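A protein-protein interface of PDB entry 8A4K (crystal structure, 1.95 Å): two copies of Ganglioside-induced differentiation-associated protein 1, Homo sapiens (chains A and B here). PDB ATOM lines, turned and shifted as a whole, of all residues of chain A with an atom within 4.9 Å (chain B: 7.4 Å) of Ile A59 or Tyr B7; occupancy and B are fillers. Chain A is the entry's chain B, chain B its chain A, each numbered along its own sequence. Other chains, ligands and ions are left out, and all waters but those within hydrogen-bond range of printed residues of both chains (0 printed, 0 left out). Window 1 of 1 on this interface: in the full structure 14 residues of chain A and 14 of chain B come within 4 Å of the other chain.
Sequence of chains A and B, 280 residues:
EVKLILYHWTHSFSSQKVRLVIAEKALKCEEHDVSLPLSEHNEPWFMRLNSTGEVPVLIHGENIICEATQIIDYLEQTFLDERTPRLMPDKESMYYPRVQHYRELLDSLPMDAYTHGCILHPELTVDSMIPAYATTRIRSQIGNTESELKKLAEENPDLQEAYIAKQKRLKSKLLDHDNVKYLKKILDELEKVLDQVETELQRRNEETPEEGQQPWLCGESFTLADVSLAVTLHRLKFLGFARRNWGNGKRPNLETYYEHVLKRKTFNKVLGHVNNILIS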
ATOM      1  N   LYS A   3       7.048 -22.713  16.870  1.00  0.00           N
ATOM      2  CA  LYS A   3       6.053 -23.760  16.924  1.00  0.00           C
ATOM      3  C   LYS A   3       4.888 -23.285  17.773  1.00  0.00           C
ATOM      4  O   LYS A   3       5.043 -22.502  18.714  1.00  0.00           O
ATOM      5  CB  LYS A   3       6.658 -25.033  17.495  1.00  0.00           C
ATOM      6  CG  LYS A   3       6.017 -26.271  16.936  1.00  0.00           C
ATOM      7  CD  LYS A   3       6.542 -27.529  17.623  1.00  0.00           C
ATOM      8  CE  LYS A   3       8.037 -27.750  17.376  1.00  0.00           C
ATOM      9  NZ  LYS A   3       8.441 -29.103  17.895  1.00  0.00           N
ATOM     10  N   LEU A   4       3.715 -23.729  17.411  1.00  0.00           N
ATOM     11  CA  LEU A   4       2.521 -23.533  18.217  1.00  0.00           C
ATOM     12  C   LEU A   4       2.247 -24.836  18.955  1.00  0.00           C
ATOM     13  O   LEU A   4       2.039 -25.874  18.322  1.00  0.00           O
ATOM     14  CB  LEU A   4       1.389 -23.120  17.293  1.00  0.00           C
ATOM     15  CG  LEU A   4       0.278 -22.263  17.853  1.00  0.00           C
ATOM     16  CD1 LEU A   4       0.728 -21.015  18.496  1.00  0.00           C
ATOM     17  CD2 LEU A   4      -0.649 -21.908  16.691  1.00  0.00           C
ATOM     18  N   ILE A   5       2.257 -24.792  20.284  1.00  0.00           N
ATOM     19  CA  ILE A   5       2.090 -25.996  21.083  1.00  0.00           C
ATOM     20  C   ILE A   5       0.892 -25.834  22.000  1.00  0.00           C
ATOM     21  O   ILE A   5       0.765 -24.816  22.699  1.00  0.00           O
ATOM     22  CB  ILE A   5       3.337 -26.306  21.924  1.00  0.00           C
ATOM     23  CG1 ILE A   5       4.561 -26.525  21.044  1.00  0.00           C
ATOM     24  CG2 ILE A   5       3.080 -27.547  22.763  1.00  0.00           C
ATOM     25  CD1 ILE A   5       5.838 -26.156  21.773  1.00  0.00           C
ATOM     26  N   TYR A   7      -1.268 -27.955  25.007  1.00  0.00           N
ATOM     27  CA  TYR A   7      -1.580 -29.029  25.934  1.00  0.00           C
ATOM     28  C   TYR A   7      -3.004 -28.814  26.424  1.00  0.00           C
ATOM     29  O   TYR A   7      -3.341 -27.708  26.857  1.00  0.00           O
ATOM     30  CB  TYR A   7      -0.601 -29.042  27.111  1.00  0.00           C
ATOM     31  CG  TYR A   7       0.813 -29.436  26.745  1.00  0.00           C
ATOM     32  CD1 TYR A   7       1.237 -30.760  26.852  1.00  0.00           C
ATOM     33  CD2 TYR A   7       1.748 -28.458  26.360  1.00  0.00           C
ATOM     34  CE1 TYR A   7       2.525 -31.129  26.548  1.00  0.00           C
ATOM     35  CE2 TYR A   7       3.066 -28.813  26.061  1.00  0.00           C
ATOM     36  CZ  TYR A   7       3.453 -30.152  26.167  1.00  0.00           C
ATOM     37  OH  TYR A   7       4.747 -30.524  25.883  1.00  0.00           O
ATOM     38  N   VAL A  57      -3.229 -24.862  27.849  1.00  0.00           N
ATOM     39  CA  VAL A  57      -2.126 -23.901  27.778  1.00  0.00           C
ATOM     40  C   VAL A  57      -1.501 -23.939  26.390  1.00  0.00           C
ATOM     41  O   VAL A  57      -1.238 -25.013  25.847  1.00  0.00           O
ATOM     42  CB  VAL A  57      -1.045 -24.160  28.837  1.00  0.00           C
ATOM     43  CG1 VAL A  57      -0.457 -25.527  28.611  1.00  0.00           C
ATOM     44  CG2 VAL A  57       0.091 -23.078  28.797  1.00  0.00           C
ATOM     45  N   LEU A  58      -1.266 -22.759  25.830  1.00  0.00           N
ATOM     46  CA  LEU A  58      -0.560 -22.584  24.570  1.00  0.00           C
ATOM     47  C   LEU A  58       0.879 -22.142  24.854  1.00  0.00           C
ATOM     48  O   LEU A  58       1.111 -21.209  25.631  1.00  0.00           O
ATOM     49  CB  LEU A  58      -1.232 -21.494  23.744  1.00  0.00           C
ATOM     50  CG  LEU A  58      -0.768 -21.309  22.315  1.00  0.00           C
ATOM     51  CD1 LEU A  58      -1.363 -22.430  21.433  1.00  0.00           C
ATOM     52  CD2 LEU A  58      -1.246 -19.995  21.706  1.00  0.00           C
ATOM     53  N   ILE A  59       1.836 -22.730  24.159  1.00  0.00           N
ATOM     54  CA  ILE A  59       3.188 -22.192  24.109  1.00  0.00           C
ATOM     55  C   ILE A  59       3.447 -21.774  22.668  1.00  0.00           C
ATOM     56  O   ILE A  59       3.196 -22.553  21.742  1.00  0.00           O
ATOM     57  CB  ILE A  59       4.222 -23.213  24.592  1.00  0.00           C
ATOM     58  CG1 ILE A  59       3.915 -23.683  26.031  1.00  0.00           C
ATOM     59  CG2 ILE A  59       5.581 -22.627  24.504  1.00  0.00           C
ATOM     60  CD1 ILE A  59       3.523 -25.091  26.051  1.00  0.00           C
ATOM     61  N   HIS A  60       3.910 -20.529  22.476  1.00  0.00           N
ATOM     62  CA  HIS A  60       4.185 -19.993  21.131  1.00  0.00           C
ATOM     63  C   HIS A  60       5.466 -19.194  21.223  1.00  0.00           C
ATOM     64  O   HIS A  60       5.437 -18.054  21.695  1.00  0.00           O
ATOM     65  CB  HIS A  60       3.084 -19.097  20.591  1.00  0.00           C
ATOM     66  CG  HIS A  60       3.383 -18.523  19.238  1.00  0.00           C
ATOM     67  ND1 HIS A  60       3.077 -17.223  18.905  1.00  0.00           N
ATOM     68  CD2 HIS A  60       4.005 -19.051  18.156  1.00  0.00           C
ATOM     69  CE1 HIS A  60       3.444 -16.992  17.657  1.00  0.00           C
ATOM     70  NE2 HIS A  60       4.026 -18.081  17.187  1.00  0.00           N
ATOM     71  N   GLY A  61       6.563 -19.796  20.811  1.00  0.00           N
ATOM     72  CA  GLY A  61       7.846 -19.169  21.026  1.00  0.00           C
ATOM     73  C   GLY A  61       8.011 -18.907  22.499  1.00  0.00           C
ATOM     74  O   GLY A  61       7.990 -19.823  23.320  1.00  0.00           O
ATOM     75  N   ASN A  63       5.994 -17.099  24.424  1.00  0.00           N
ATOM     76  CA  ASN A  63       4.774 -16.743  25.133  1.00  0.00           C
ATOM     77  C   ASN A  63       4.088 -18.013  25.635  1.00  0.00           C
ATOM     78  O   ASN A  63       4.009 -19.002  24.910  1.00  0.00           O
ATOM     79  CB  ASN A  63       3.868 -15.931  24.208  1.00  0.00           C
ATOM     80  CG  ASN A  63       4.471 -14.599  23.849  1.00  0.00           C
ATOM     81  OD1 ASN A  63       5.089 -13.947  24.676  1.00  0.00           O
ATOM     82  ND2 ASN A  63       4.320 -14.191  22.576  1.00  0.00           N
ATOM     83  N   ILE A  64       3.623 -17.964  26.882  1.00  0.00           N
ATOM     84  CA  ILE A  64       2.915 -19.046  27.561  1.00  0.00           C
ATOM     85  C   ILE A  64       1.599 -18.442  28.021  1.00  0.00           C
ATOM     86  O   ILE A  64       1.605 -17.427  28.755  1.00  0.00           O
ATOM     87  CB  ILE A  64       3.690 -19.546  28.781  1.00  0.00           C
ATOM     88  CG1 ILE A  64       5.012 -20.135  28.294  1.00  0.00           C
ATOM     89  CG2 ILE A  64       2.872 -20.693  29.553  1.00  0.00           C
ATOM     90  CD1 ILE A  64       5.994 -20.536  29.360  1.00  0.00           C
ATOM     91  N   ILE B   5       7.013 -31.820  33.136  1.00  0.00           N
ATOM     92  CA  ILE B   5       7.431 -30.892  32.099  1.00  0.00           C
ATOM     93  C   ILE B   5       7.158 -29.475  32.572  1.00  0.00           C
ATOM     94  O   ILE B   5       6.037 -29.155  33.000  1.00  0.00           O
ATOM     95  CB  ILE B   5       6.720 -31.157  30.764  1.00  0.00           C
ATOM     96  CG1 ILE B   5       7.039 -32.555  30.266  1.00  0.00           C
ATOM     97  CG2 ILE B   5       7.168 -30.151  29.726  1.00  0.00           C
ATOM     98  CD1 ILE B   5       5.932 -33.179  29.440  1.00  0.00           C
ATOM     99  N   LEU B   6       8.165 -28.617  32.439  1.00  0.00           N
ATOM    100  CA  LEU B   6       8.075 -27.238  32.877  1.00  0.00           C
ATOM    101  C   LEU B   6       8.453 -26.338  31.718  1.00  0.00           C
ATOM    102  O   LEU B   6       9.559 -26.440  31.169  1.00  0.00           O
ATOM    103  CB  LEU B   6       8.986 -26.956  34.077  1.00  0.00           C
ATOM    104  CG  LEU B   6       8.931 -25.504  34.545  1.00  0.00           C
ATOM    105  CD1 LEU B   6       7.590 -25.158  35.126  1.00  0.00           C
ATOM    106  CD2 LEU B   6      10.106 -25.231  35.557  1.00  0.00           C
ATOM    107  N   TYR B   7       7.538 -25.459  31.348  1.00  0.00           N
ATOM    108  CA  TYR B   7       7.850 -24.373  30.443  1.00  0.00           C
ATOM    109  C   TYR B   7       7.938 -23.097  31.261  1.00  0.00           C
ATOM    110  O   TYR B   7       7.048 -22.808  32.065  1.00  0.00           O
ATOM    111  CB  TYR B   7       6.789 -24.245  29.377  1.00  0.00           C
ATOM    112  CG  TYR B   7       6.723 -25.364  28.372  1.00  0.00           C
ATOM    113  CD1 TYR B   7       7.461 -25.298  27.193  1.00  0.00           C
ATOM    114  CD2 TYR B   7       5.911 -26.487  28.587  1.00  0.00           C
ATOM    115  CE1 TYR B   7       7.394 -26.310  26.248  1.00  0.00           C
ATOM    116  CE2 TYR B   7       5.810 -27.497  27.636  1.00  0.00           C
ATOM    117  CZ  TYR B   7       6.566 -27.419  26.472  1.00  0.00           C
ATOM    118  OH  TYR B   7       6.469 -28.434  25.523  1.00  0.00           O
ATOM    119  N   HIS B   8       9.004 -22.326  31.048  1.00  0.00           N
ATOM    120  CA  HIS B   8       9.336 -21.221  31.934  1.00  0.00           C
ATOM    121  C   HIS B   8      10.299 -20.262  31.225  1.00  0.00           C
ATOM    122  O   HIS B   8      10.972 -20.625  30.254  1.00  0.00           O
ATOM    123  CB  HIS B   8       9.979 -21.731  33.218  1.00  0.00           C
ATOM    124  CG  HIS B   8      11.364 -22.243  32.979  1.00  0.00           C
ATOM    125  ND1 HIS B   8      12.497 -21.489  33.243  1.00  0.00           N
ATOM    126  CD2 HIS B   8      11.792 -23.369  32.359  1.00  0.00           C
ATOM    127  CE1 HIS B   8      13.565 -22.157  32.841  1.00  0.00           C
ATOM    128  NE2 HIS B   8      13.166 -23.296  32.304  1.00  0.00           N
ATOM    129  N   TRP B   9      10.387 -19.038  31.759  1.00  0.00           N
ATOM    130  CA  TRP B   9      11.445 -18.094  31.410  1.00  0.00           C
ATOM    131  C   TRP B   9      12.483 -18.095  32.523  1.00  0.00           C
ATOM    132  O   TRP B   9      12.186 -17.664  33.647  1.00  0.00           O
ATOM    133  CB  TRP B   9      10.922 -16.678  31.267  1.00  0.00           C
ATOM    134  CG  TRP B   9      10.201 -16.271  30.050  1.00  0.00           C
ATOM    135  CD1 TRP B   9       9.195 -16.925  29.405  1.00  0.00           C
ATOM    136  CD2 TRP B   9      10.402 -15.028  29.340  1.00  0.00           C
ATOM    137  NE1 TRP B   9       8.769 -16.174  28.320  1.00  0.00           N
ATOM    138  CE2 TRP B   9       9.488 -15.002  28.270  1.00  0.00           C
ATOM    139  CE3 TRP B   9      11.257 -13.938  29.520  1.00  0.00           C
ATOM    140  CZ2 TRP B   9       9.414 -13.909  27.361  1.00  0.00           C
ATOM    141  CZ3 TRP B   9      11.193 -12.864  28.624  1.00  0.00           C
ATOM    142  CH2 TRP B   9      10.292 -12.861  27.554  1.00  0.00           C
ATOM    143  N   SER B  15       9.717 -18.350  37.666  1.00  0.00           N
ATOM    144  CA  SER B  15      10.431 -19.564  37.249  1.00  0.00           C
ATOM    145  C   SER B  15      11.505 -19.911  38.248  1.00  0.00           C
ATOM    146  O   SER B  15      11.789 -21.088  38.503  1.00  0.00           O
ATOM    147  CB  SER B  15      11.057 -19.371  35.845  1.00  0.00           C
ATOM    148  OG  SER B  15      12.138 -20.286  35.659  1.00  0.00           O
ATOM    149  N   VAL B  18       9.956 -21.762  41.168  1.00  0.00           N
ATOM    150  CA  VAL B  18       9.549 -23.112  40.775  1.00  0.00           C
ATOM    151  C   VAL B  18      10.762 -24.028  40.621  1.00  0.00           C
ATOM    152  O   VAL B  18      10.765 -25.163  41.074  1.00  0.00           O
ATOM    153  CB  VAL B  18       8.730 -23.071  39.467  1.00  0.00           C
ATOM    154  CG1 VAL B  18       8.545 -24.468  38.970  1.00  0.00           C
ATOM    155  CG2 VAL B  18       7.406 -22.385  39.684  1.00  0.00           C
ATOM    156  N   CYS B  29      12.861 -33.291  36.149  1.00  0.00           N
ATOM    157  CA  CYS B  29      11.987 -32.421  35.381  1.00  0.00           C
ATOM    158  C   CYS B  29      12.598 -32.086  34.033  1.00  0.00           C
ATOM    159  O   CYS B  29      13.771 -31.729  33.953  1.00  0.00           O
ATOM    160  CB  CYS B  29      11.691 -31.122  36.134  1.00  0.00           C
ATOM    161  SG  CYS B  29      10.490 -30.048  35.284  1.00  0.00           S
ATOM    162  N   GLU B  30      11.788 -32.187  32.989  1.00  0.00           N
ATOM    163  CA  GLU B  30      12.173 -31.765  31.648  1.00  0.00           C
ATOM    164  C   GLU B  30      11.798 -30.292  31.541  1.00  0.00           C
ATOM    165  O   GLU B  30      10.624 -29.952  31.401  1.00  0.00           O
ATOM    166  CB  GLU B  30      11.479 -32.627  30.602  1.00  0.00           C
ATOM    167  CG  GLU B  30      11.919 -32.347  29.171  1.00  0.00           C
ATOM    168  CD  GLU B  30      11.174 -33.205  28.165  1.00  0.00           C
ATOM    169  OE1 GLU B  30      11.551 -34.387  27.998  1.00  0.00           O
ATOM    170  OE2 GLU B  30      10.196 -32.722  27.568  1.00  0.00           O
ATOM    171  N   GLU B  31      12.797 -29.417  31.619  1.00  0.00           N
ATOM    172  CA  GLU B  31      12.581 -27.982  31.751  1.00  0.00           C
ATOM    173  C   GLU B  31      12.855 -27.322  30.416  1.00  0.00           C
ATOM    174  O   GLU B  31      13.951 -27.486  29.861  1.00  0.00           O
ATOM    175  CB  GLU B  31      13.501 -27.374  32.816  1.00  0.00           C
ATOM    176  CG  GLU B  31      13.299 -27.980  34.210  1.00  0.00           C
ATOM    177  CD  GLU B  31      14.160 -27.382  35.336  1.00  0.00           C
ATOM    178  OE1 GLU B  31      15.055 -26.529  35.111  1.00  0.00           O
ATOM    179  OE2 GLU B  31      13.891 -27.783  36.489  1.00  0.00           O
ATOM    180  N   HIS B  32      11.888 -26.529  29.932  1.00  0.00           N
ATOM    181  CA  HIS B  32      12.047 -25.797  28.689  1.00  0.00           C
ATOM    182  C   HIS B  32      12.061 -24.293  28.945  1.00  0.00           C
ATOM    183  O   HIS B  32      11.013 -23.682  29.181  1.00  0.00           O
ATOM    184  CB  HIS B  32      10.938 -26.142  27.703  1.00  0.00           C
ATOM    185  CG  HIS B  32      10.831 -27.598  27.405  1.00  0.00           C
ATOM    186  ND1 HIS B  32      11.697 -28.232  26.550  1.00  0.00           N
ATOM    187  CD2 HIS B  32       9.934 -28.531  27.798  1.00  0.00           C
ATOM    188  CE1 HIS B  32      11.374 -29.509  26.464  1.00  0.00           C
ATOM    189  NE2 HIS B  32      10.294 -29.713  27.196  1.00  0.00           N
ATOM    190  N   ASP B  33      13.259 -23.703  28.880  1.00  0.00           N
ATOM    191  CA  ASP B  33      13.422 -22.254  28.848  1.00  0.00           C
ATOM    192  C   ASP B  33      12.967 -21.760  27.483  1.00  0.00           C
ATOM    193  O   ASP B  33      13.616 -22.033  26.476  1.00  0.00           O
ATOM    194  CB  ASP B  33      14.889 -21.920  29.108  1.00  0.00           C
ATOM    195  CG  ASP B  33      15.199 -20.429  29.090  1.00  0.00           C
ATOM    196  OD1 ASP B  33      14.277 -19.560  29.173  1.00  0.00           O
ATOM    197  OD2 ASP B  33      16.429 -20.139  29.057  1.00  0.00           O
ATOM    198  N   VAL B  34      11.831 -21.058  27.439  1.00  0.00           N
ATOM    199  CA  VAL B  34      11.319 -20.570  26.174  1.00  0.00           C
ATOM    200  C   VAL B  34      11.840 -19.186  25.847  1.00  0.00           C
ATOM    201  O   VAL B  34      11.503 -18.646  24.788  1.00  0.00           O
ATOM    202  CB  VAL B  34       9.788 -20.518  26.194  1.00  0.00           C
ATOM    203  CG1 VAL B  34       9.252 -21.867  26.614  1.00  0.00           C
ATOM    204  CG2 VAL B  34       9.285 -19.457  27.140  1.00  0.00           C
ATOM    205  N   VAL B  55       4.454 -16.337  33.490  1.00  0.00           N
ATOM    206  CA  VAL B  55       3.625 -17.477  33.885  1.00  0.00           C
ATOM    207  C   VAL B  55       4.249 -18.797  33.440  1.00  0.00           C
ATOM    208  O   VAL B  55       4.072 -19.229  32.304  1.00  0.00           O
ATOM    209  CB  VAL B  55       2.206 -17.325  33.344  1.00  0.00           C
ATOM    210  CG1 VAL B  55       1.441 -18.619  33.522  1.00  0.00           C
ATOM    211  CG2 VAL B  55       1.533 -16.150  34.055  1.00  0.00           C
ATOM    212  N   PRO B  56       4.963 -19.474  34.300  1.00  0.00           N
ATOM    213  CA  PRO B  56       5.380 -20.834  33.968  1.00  0.00           C
ATOM    214  C   PRO B  56       4.178 -21.788  34.030  1.00  0.00           C
ATOM    215  O   PRO B  56       3.092 -21.467  34.536  1.00  0.00           O
ATOM    216  CB  PRO B  56       6.405 -21.146  35.048  1.00  0.00           C
ATOM    217  CG  PRO B  56       5.902 -20.362  36.233  1.00  0.00           C
ATOM    218  CD  PRO B  56       5.260 -19.120  35.703  1.00  0.00           C
ATOM    219  N   VAL B  57       4.359 -22.933  33.412  1.00  0.00           N
ATOM    220  CA  VAL B  57       3.326 -23.941  33.385  1.00  0.00           C
ATOM    221  C   VAL B  57       4.013 -25.270  33.520  1.00  0.00           C
ATOM    222  O   VAL B  57       5.042 -25.526  32.875  1.00  0.00           O
ATOM    223  CB  VAL B  57       2.491 -23.923  32.101  1.00  0.00           C
ATOM    224  CG1 VAL B  57       3.350 -24.170  30.938  1.00  0.00           C
ATOM    225  CG2 VAL B  57       1.421 -25.027  32.144  1.00  0.00           C
ATOM    226  N   LEU B  58       3.441 -26.099  34.386  1.00  0.00           N
ATOM    227  CA  LEU B  58       3.840 -27.465  34.618  1.00  0.00           C
ATOM    228  C   LEU B  58       2.828 -28.411  33.981  1.00  0.00           C
ATOM    229  O   LEU B  58       1.606 -28.279  34.186  1.00  0.00           O
ATOM    230  CB  LEU B  58       3.895 -27.748  36.118  1.00  0.00           C
ATOM    231  CG  LEU B  58       4.466 -29.112  36.491  1.00  0.00           C
ATOM    232  CD1 LEU B  58       6.029 -29.022  36.385  1.00  0.00           C
ATOM    233  CD2 LEU B  58       4.044 -29.550  37.870  1.00  0.00           C
ATOM    234  N   ILE B  59       3.340 -29.430  33.296  1.00  0.00           N
ATOM    235  CA  ILE B  59       2.514 -30.551  32.847  1.00  0.00           C
ATOM    236  C   ILE B  59       3.015 -31.819  33.516  1.00  0.00           C
ATOM    237  O   ILE B  59       4.205 -32.138  33.425  1.00  0.00           O
ATOM    238  CB  ILE B  59       2.554 -30.686  31.319  1.00  0.00           C
ATOM    239  CG1 ILE B  59       2.158 -29.340  30.671  1.00  0.00           C
ATOM    240  CG2 ILE B  59       1.597 -31.753  30.831  1.00  0.00           C
ATOM    241  CD1 ILE B  59       3.296 -28.704  29.993  1.00  0.00           C
ATOM    242  N   ILE B  65      -0.871 -27.099  35.244  1.00  0.00           N
ATOM    243  CA  ILE B  65      -0.905 -26.147  36.342  1.00  0.00           C
ATOM    244  C   ILE B  65      -0.074 -24.949  35.901  1.00  0.00           C
ATOM    245  O   ILE B  65       1.134 -25.080  35.639  1.00  0.00           O
ATOM    246  CB  ILE B  65      -0.354 -26.707  37.663  1.00  0.00           C
ATOM    247  CG1 ILE B  65      -0.949 -28.069  38.021  1.00  0.00           C
ATOM    248  CG2 ILE B  65      -0.656 -25.814  38.860  1.00  0.00           C
ATOM    249  CD1 ILE B  65      -0.007 -29.174  37.569  1.00  0.00           C
ATOM    250  N   ILE B  71       1.797 -24.132  40.957  1.00  0.00           N
ATOM    251  CA  ILE B  71       2.719 -25.219  40.628  1.00  0.00           C
ATOM    252  C   ILE B  71       3.378 -25.747  41.889  1.00  0.00           C
ATOM    253  O   ILE B  71       3.532 -26.961  42.081  1.00  0.00           O
ATOM    254  CB  ILE B  71       3.786 -24.713  39.623  1.00  0.00           C
ATOM    255  CG1 ILE B  71       3.145 -24.447  38.280  1.00  0.00           C
ATOM    256  CG2 ILE B  71       4.941 -25.718  39.553  1.00  0.00           C
ATOM    257  CD1 ILE B  71       4.000 -23.749  37.298  1.00  0.00           C
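N of Val B34 lies within hydrogen-bond range of O of His B8.
The backbone NH (N) of Val A57 is in hydrogen-bond range of the backbone carbonyl oxygen (O) of Tyr A7.
The backbone NH (N) of Ile A59 sits at hydrogen-bond distance from the backbone carbonyl oxygen (O) of Ile A5, at 2.8 Å.
A ring nitrogen (NE2) of His B8 sits at hydrogen-bond distance from the backbone NH (N) of Asp B33, at 3.4 Å.
O of His B32 is in hydrogen-bond range of N of His B8, at 3.1 Å.
The backbone carbonyl oxygen (O) of Ile B5 is in hydrogen-bond range of the backbone NH (N) of Ile B59 (2.7 Å).
CD1 of Ile B59 touches CE2 of Tyr A7 (3.9 Å).
CE2 of Tyr B7 touches CD1 of Ile A59, 3.7 Å away.
Val B34 touches Gly A61.
Ile A64 touches Tyr B7 (CD1 to O, 3.7 Å).
Ile A64 touches His B8 (CD1 to N, 3.9 Å).
CG2 of Ile A64 touches O of Val B55 (3.3 Å).
CG2 of Ile A64 touches CG1 of Val B57 (3.8 Å).
Hydrophobic or aromatic side chains of chain B within 4 Å of the printed part of chain A: Tyr B7, Val B34, Val B57 and Ile B59.
Printed residues of chain A that touch a printed residue of chain B: Tyr A7, Ile A59, Gly A61 and Ile A64.
Hydrophobic or aromatic side chains of chain A that line the printed part of chain B: Tyr A7, Ile A59 and Ile A64.
Among the printed residues, no Asp or Glu carboxylate lies within 4 Å of a Lys or Arg side-chain nitrogen of the other chain.
Tyr A7 touches its own counterpart, Tyr B7.
Tyr A7 touches Ile B59, and with the chains exchanged Ile A59 touches Tyr B7.
Of the 8 pairs that touch across the chains among the printed residues, 3 have their exchanged pair printed and touching as well.
OH of Tyr B7 is in hydrogen-bond range of OH of Tyr A7.
Ile A59 touches one residue of chain B.
Tyr B7 touches just these residues of chain A: Tyr A7, Ile A59 and Ile A64.
Of the printed residues of chain B, Tyr A7 touches Tyr B7 and Ile B59.
Of the printed residues of chain B, Gly A61 touches Val B34 (3.5 Å).
Of the printed residues of chain B, Ile A64 touches Tyr B7 (3.7 Å), His B8 (3.9 Å), Val B55 (3.3 Å) and Val B57 (3.8 Å).
Ile B71 touches none of the printed residues of chain A.
Leu A58 touches none of the printed residues of chain B.
The nearest residue of chain B that does not touch Ile A59 is Val B34 (4.3 Å).
The nearest printed residue of chain A that does not touch Val B55 is Val A57 (6.6 Å).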
